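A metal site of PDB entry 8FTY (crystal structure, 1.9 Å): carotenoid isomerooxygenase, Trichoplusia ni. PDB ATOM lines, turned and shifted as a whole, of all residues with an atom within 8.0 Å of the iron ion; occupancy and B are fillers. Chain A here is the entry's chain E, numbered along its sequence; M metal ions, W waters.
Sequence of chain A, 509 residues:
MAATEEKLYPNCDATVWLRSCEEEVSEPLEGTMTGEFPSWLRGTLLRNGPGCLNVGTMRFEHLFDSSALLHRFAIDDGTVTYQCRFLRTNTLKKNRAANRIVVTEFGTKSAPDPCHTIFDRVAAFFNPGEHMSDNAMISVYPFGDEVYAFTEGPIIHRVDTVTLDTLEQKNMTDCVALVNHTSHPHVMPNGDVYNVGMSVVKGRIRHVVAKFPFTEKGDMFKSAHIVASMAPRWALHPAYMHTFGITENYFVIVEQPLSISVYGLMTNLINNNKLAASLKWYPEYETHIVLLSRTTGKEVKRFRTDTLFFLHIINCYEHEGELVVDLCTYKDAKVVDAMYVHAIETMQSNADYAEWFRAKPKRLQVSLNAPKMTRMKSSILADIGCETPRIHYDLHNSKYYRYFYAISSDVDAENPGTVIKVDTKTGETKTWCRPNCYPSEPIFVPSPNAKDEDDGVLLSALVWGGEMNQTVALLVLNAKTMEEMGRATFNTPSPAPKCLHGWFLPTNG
A ring nitrogen (ND1) of His 312 lies within hydrogen-bond range of the side-chain carboxylate (OE1) of Glu 387 (2.8 Å).
ND1 of His 501 is in hydrogen-bond range of OE2 of Glu 441, 2.8 Å away.
A ring nitrogen (ND1) of His 184 is in hydrogen-bond range of the side-chain hydroxyl (OH) of Tyr 141 (2.8 Å).
A ring nitrogen (ND1) of His 242 sits at hydrogen-bond distance from the side-chain carboxylate of Glu 152 (2.9 Å).
ND1 of His 242 sits at hydrogen-bond distance from OH of Tyr 240 (3.4 Å).
Of the 17 residues printed, 4 come within 4 Å of the iron ion.
Along chain A the residues within 4 Å of the iron ion span positions 184 to 501.
The nearest printed residue that does not touch the iron ion is Ile 138 (4.2 Å).
The iron ion is bound by NE2 of His 312, 2.1 Å away.
The iron ion is bound by NE2 of His 501, at 2.2 Å.
The iron ion is bound by a ring nitrogen (NE2) of His 184 (2.2 Å).
The iron ion is bound by NE2 of His 242, at 2.2 Å.
Water W1 binds the iron ion (2.3 Å).
The iron ion has five donor atoms within binding distance.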
ATOM      1  N   ILE A 138     -21.653 -22.148  20.573  1.00  0.00           N
ATOM      2  CA  ILE A 138     -21.975 -22.664  21.903  1.00  0.00           C
ATOM      3  C   ILE A 138     -22.305 -21.526  22.864  1.00  0.00           C
ATOM      4  O   ILE A 138     -23.343 -21.571  23.516  1.00  0.00           O
ATOM      5  CB  ILE A 138     -20.846 -23.557  22.438  1.00  0.00           C
ATOM      6  CG1 ILE A 138     -20.618 -24.768  21.527  1.00  0.00           C
ATOM      7  CG2 ILE A 138     -21.128 -23.966  23.871  1.00  0.00           C
ATOM      8  CD1 ILE A 138     -19.467 -25.646  21.930  1.00  0.00           C
ATOM      9  N   SER A 139     -21.433 -20.513  22.961  1.00  0.00           N
ATOM     10  CA  SER A 139     -21.521 -19.549  24.056  1.00  0.00           C
ATOM     11  C   SER A 139     -20.949 -18.193  23.660  1.00  0.00           C
ATOM     12  O   SER A 139     -20.366 -18.046  22.593  1.00  0.00           O
ATOM     13  CB  SER A 139     -20.800 -20.067  25.265  1.00  0.00           C
ATOM     14  OG  SER A 139     -19.424 -20.241  24.987  1.00  0.00           O
ATOM     15  N   TYR A 141     -18.877 -14.933  25.935  1.00  0.00           N
ATOM     16  CA  TYR A 141     -18.262 -14.587  27.204  1.00  0.00           C
ATOM     17  C   TYR A 141     -17.577 -13.230  27.123  1.00  0.00           C
ATOM     18  O   TYR A 141     -16.991 -12.893  26.098  1.00  0.00           O
ATOM     19  CB  TYR A 141     -17.242 -15.649  27.627  1.00  0.00           C
ATOM     20  CG  TYR A 141     -17.834 -16.837  28.341  1.00  0.00           C
ATOM     21  CD1 TYR A 141     -18.391 -17.897  27.640  1.00  0.00           C
ATOM     22  CD2 TYR A 141     -17.881 -16.880  29.720  1.00  0.00           C
ATOM     23  CE1 TYR A 141     -18.942 -18.976  28.292  1.00  0.00           C
ATOM     24  CE2 TYR A 141     -18.437 -17.960  30.401  1.00  0.00           C
ATOM     25  CZ  TYR A 141     -18.973 -19.015  29.675  1.00  0.00           C
ATOM     26  OH  TYR A 141     -19.528 -20.083  30.334  1.00  0.00           O
ATOM     27  N   GLU A 152     -15.090 -25.103  20.631  1.00  0.00           N
ATOM     28  CA  GLU A 152     -14.038 -25.789  21.379  1.00  0.00           C
ATOM     29  C   GLU A 152     -12.793 -25.972  20.522  1.00  0.00           C
ATOM     30  O   GLU A 152     -11.750 -26.366  21.039  1.00  0.00           O
ATOM     31  CB  GLU A 152     -14.601 -27.068  21.988  1.00  0.00           C
ATOM     32  CG  GLU A 152     -15.873 -26.791  22.785  1.00  0.00           C
ATOM     33  CD  GLU A 152     -16.262 -27.803  23.830  1.00  0.00           C
ATOM     34  OE1 GLU A 152     -16.240 -28.995  23.523  1.00  0.00           O
ATOM     35  OE2 GLU A 152     -16.637 -27.371  24.944  1.00  0.00           O
ATOM     36  N   SER A 183     -15.684 -24.335  25.959  1.00  0.00           N
ATOM     37  CA  SER A 183     -16.502 -23.198  25.554  1.00  0.00           C
ATOM     38  C   SER A 183     -17.113 -22.511  26.781  1.00  0.00           C
ATOM     39  O   SER A 183     -18.058 -21.733  26.645  1.00  0.00           O
ATOM     40  CB  SER A 183     -17.552 -23.653  24.574  1.00  0.00           C
ATOM     41  OG  SER A 183     -18.192 -24.835  25.027  1.00  0.00           O
ATOM     42  N   HIS A 184     -16.545 -22.784  27.961  1.00  0.00           N
ATOM     43  CA  HIS A 184     -17.041 -22.252  29.213  1.00  0.00           C
ATOM     44  C   HIS A 184     -15.881 -21.786  30.077  1.00  0.00           C
ATOM     45  O   HIS A 184     -15.606 -22.356  31.128  1.00  0.00           O
ATOM     46  CB  HIS A 184     -17.904 -23.287  29.930  1.00  0.00           C
ATOM     47  CG  HIS A 184     -19.203 -23.542  29.254  1.00  0.00           C
ATOM     48  ND1 HIS A 184     -20.163 -22.566  29.149  1.00  0.00           N
ATOM     49  CD2 HIS A 184     -19.715 -24.612  28.640  1.00  0.00           C
ATOM     50  CE1 HIS A 184     -21.221 -23.042  28.513  1.00  0.00           C
ATOM     51  NE2 HIS A 184     -20.960 -24.290  28.191  1.00  0.00           N
ATOM     52  N   TYR A 240     -12.120 -35.616  27.285  1.00  0.00           N
ATOM     53  CA  TYR A 240     -12.944 -34.506  26.849  1.00  0.00           C
ATOM     54  C   TYR A 240     -13.524 -33.788  28.069  1.00  0.00           C
ATOM     55  O   TYR A 240     -13.957 -34.447  29.021  1.00  0.00           O
ATOM     56  CB  TYR A 240     -14.098 -34.983  25.965  1.00  0.00           C
ATOM     57  CG  TYR A 240     -15.060 -33.869  25.647  1.00  0.00           C
ATOM     58  CD1 TYR A 240     -14.698 -32.856  24.777  1.00  0.00           C
ATOM     59  CD2 TYR A 240     -16.298 -33.780  26.273  1.00  0.00           C
ATOM     60  CE1 TYR A 240     -15.546 -31.803  24.501  1.00  0.00           C
ATOM     61  CE2 TYR A 240     -17.165 -32.731  26.007  1.00  0.00           C
ATOM     62  CZ  TYR A 240     -16.790 -31.737  25.118  1.00  0.00           C
ATOM     63  OH  TYR A 240     -17.614 -30.687  24.846  1.00  0.00           O
ATOM     64  N   HIS A 242     -16.137 -30.273  28.828  1.00  0.00           N
ATOM     65  CA  HIS A 242     -16.943 -29.151  28.352  1.00  0.00           C
ATOM     66  C   HIS A 242     -16.843 -27.987  29.330  1.00  0.00           C
ATOM     67  O   HIS A 242     -16.962 -26.832  28.935  1.00  0.00           O
ATOM     68  CB  HIS A 242     -18.380 -29.610  28.127  1.00  0.00           C
ATOM     69  CG  HIS A 242     -19.291 -28.571  27.573  1.00  0.00           C
ATOM     70  ND1 HIS A 242     -19.082 -27.966  26.347  1.00  0.00           N
ATOM     71  CD2 HIS A 242     -20.416 -28.041  28.059  1.00  0.00           C
ATOM     72  CE1 HIS A 242     -20.049 -27.094  26.123  1.00  0.00           C
ATOM     73  NE2 HIS A 242     -20.883 -27.118  27.153  1.00  0.00           N
ATOM     74  N   THR A 243     -16.664 -28.308  30.615  1.00  0.00           N
ATOM     75  CA  THR A 243     -16.497 -27.300  31.652  1.00  0.00           C
ATOM     76  C   THR A 243     -15.388 -27.735  32.619  1.00  0.00           C
ATOM     77  O   THR A 243     -14.933 -28.885  32.581  1.00  0.00           O
ATOM     78  CB  THR A 243     -17.802 -27.048  32.428  1.00  0.00           C
ATOM     79  OG1 THR A 243     -18.342 -28.283  32.898  1.00  0.00           O
ATOM     80  CG2 THR A 243     -18.856 -26.352  31.585  1.00  0.00           C
ATOM     81  N   LEU A 311     -21.541 -32.439  31.136  1.00  0.00           N
ATOM     82  CA  LEU A 311     -21.284 -31.261  30.330  1.00  0.00           C
ATOM     83  C   LEU A 311     -21.004 -30.075  31.256  1.00  0.00           C
ATOM     84  O   LEU A 311     -19.965 -29.431  31.116  1.00  0.00           O
ATOM     85  CB  LEU A 311     -22.503 -30.991  29.438  1.00  0.00           C
ATOM     86  CG  LEU A 311     -22.768 -32.026  28.347  1.00  0.00           C
ATOM     87  CD1 LEU A 311     -24.050 -31.680  27.596  1.00  0.00           C
ATOM     88  CD2 LEU A 311     -21.614 -32.118  27.381  1.00  0.00           C
ATOM     89  N   HIS A 312     -21.926 -29.810  32.191  1.00  0.00           N
ATOM     90  CA  HIS A 312     -21.944 -28.564  32.940  1.00  0.00           C
ATOM     91  C   HIS A 312     -21.729 -28.793  34.428  1.00  0.00           C
ATOM     92  O   HIS A 312     -22.563 -29.404  35.090  1.00  0.00           O
ATOM     93  CB  HIS A 312     -23.243 -27.808  32.664  1.00  0.00           C
ATOM     94  CG  HIS A 312     -23.403 -27.436  31.226  1.00  0.00           C
ATOM     95  ND1 HIS A 312     -24.355 -28.009  30.406  1.00  0.00           N
ATOM     96  CD2 HIS A 312     -22.702 -26.585  30.466  1.00  0.00           C
ATOM     97  CE1 HIS A 312     -24.227 -27.507  29.190  1.00  0.00           C
ATOM     98  NE2 HIS A 312     -23.227 -26.638  29.200  1.00  0.00           N
ATOM     99  N   GLU A 387     -30.374 -29.288  33.262  1.00  0.00           N
ATOM    100  CA  GLU A 387     -29.290 -28.939  32.360  1.00  0.00           C
ATOM    101  C   GLU A 387     -29.191 -27.430  32.202  1.00  0.00           C
ATOM    102  O   GLU A 387     -30.078 -26.697  32.623  1.00  0.00           O
ATOM    103  CB  GLU A 387     -29.460 -29.622  30.993  1.00  0.00           C
ATOM    104  CG  GLU A 387     -28.593 -30.854  30.822  1.00  0.00           C
ATOM    105  CD  GLU A 387     -27.087 -30.629  30.902  1.00  0.00           C
ATOM    106  OE1 GLU A 387     -26.658 -29.474  31.157  1.00  0.00           O
ATOM    107  OE2 GLU A 387     -26.346 -31.612  30.714  1.00  0.00           O
ATOM    108  N   THR A 388     -28.087 -26.997  31.565  1.00  0.00           N
ATOM    109  CA  THR A 388     -27.698 -25.603  31.408  1.00  0.00           C
ATOM    110  C   THR A 388     -27.935 -24.853  32.715  1.00  0.00           C
ATOM    111  O   THR A 388     -28.752 -23.930  32.772  1.00  0.00           O
ATOM    112  CB  THR A 388     -28.386 -24.943  30.209  1.00  0.00           C
ATOM    113  OG1 THR A 388     -29.786 -24.859  30.466  1.00  0.00           O
ATOM    114  CG2 THR A 388     -28.138 -25.695  28.912  1.00  0.00           C
ATOM    115  N   PRO A 389     -27.220 -25.219  33.804  1.00  0.00           N
ATOM    116  CA  PRO A 389     -27.367 -24.554  35.090  1.00  0.00           C
ATOM    117  C   PRO A 389     -26.660 -23.195  35.136  1.00  0.00           C
ATOM    118  O   PRO A 389     -25.662 -23.003  34.458  1.00  0.00           O
ATOM    119  CB  PRO A 389     -26.704 -25.549  36.059  1.00  0.00           C
ATOM    120  CG  PRO A 389     -25.598 -26.148  35.223  1.00  0.00           C
ATOM    121  CD  PRO A 389     -26.203 -26.280  33.838  1.00  0.00           C
ATOM    122  N   GLU A 441     -31.778 -21.724  29.057  1.00  0.00           N
ATOM    123  CA  GLU A 441     -30.892 -21.425  30.167  1.00  0.00           C
ATOM    124  C   GLU A 441     -31.312 -20.111  30.828  1.00  0.00           C
ATOM    125  O   GLU A 441     -31.320 -19.073  30.184  1.00  0.00           O
ATOM    126  CB  GLU A 441     -29.472 -21.317  29.617  1.00  0.00           C
ATOM    127  CG  GLU A 441     -28.451 -20.830  30.614  1.00  0.00           C
ATOM    128  CD  GLU A 441     -27.165 -20.365  29.968  1.00  0.00           C
ATOM    129  OE1 GLU A 441     -27.230 -19.434  29.153  1.00  0.00           O
ATOM    130  OE2 GLU A 441     -26.100 -20.950  30.283  1.00  0.00           O
ATOM    131  N   LEU A 500     -28.563 -21.915  22.906  1.00  0.00           N
ATOM    132  CA  LEU A 500     -27.897 -22.721  23.917  1.00  0.00           C
ATOM    133  C   LEU A 500     -27.539 -21.889  25.137  1.00  0.00           C
ATOM    134  O   LEU A 500     -28.119 -22.077  26.203  1.00  0.00           O
ATOM    135  CB  LEU A 500     -26.635 -23.360  23.318  1.00  0.00           C
ATOM    136  CG  LEU A 500     -26.839 -24.636  22.505  1.00  0.00           C
ATOM    137  CD1 LEU A 500     -25.505 -25.142  21.965  1.00  0.00           C
ATOM    138  CD2 LEU A 500     -27.515 -25.716  23.335  1.00  0.00           C
ATOM    139  N   HIS A 501     -26.558 -20.994  24.999  1.00  0.00           N
ATOM    140  CA  HIS A 501     -26.012 -20.256  26.136  1.00  0.00           C
ATOM    141  C   HIS A 501     -25.986 -18.761  25.842  1.00  0.00           C
ATOM    142  O   HIS A 501     -25.985 -18.357  24.679  1.00  0.00           O
ATOM    143  CB  HIS A 501     -24.579 -20.709  26.452  1.00  0.00           C
ATOM    144  CG  HIS A 501     -24.453 -22.077  27.030  1.00  0.00           C
ATOM    145  ND1 HIS A 501     -24.790 -22.391  28.326  1.00  0.00           N
ATOM    146  CD2 HIS A 501     -23.971 -23.212  26.493  1.00  0.00           C
ATOM    147  CE1 HIS A 501     -24.556 -23.674  28.552  1.00  0.00           C
ATOM    148  NE2 HIS A 501     -24.056 -24.191  27.452  1.00  0.00           N
HETATM  149 FE    FE M   1     -22.477 -25.653  27.481  1.00  0.00          FE
HETATM  150  O   HOH W   1     -23.352 -26.557  25.594  1.00  0.00           O
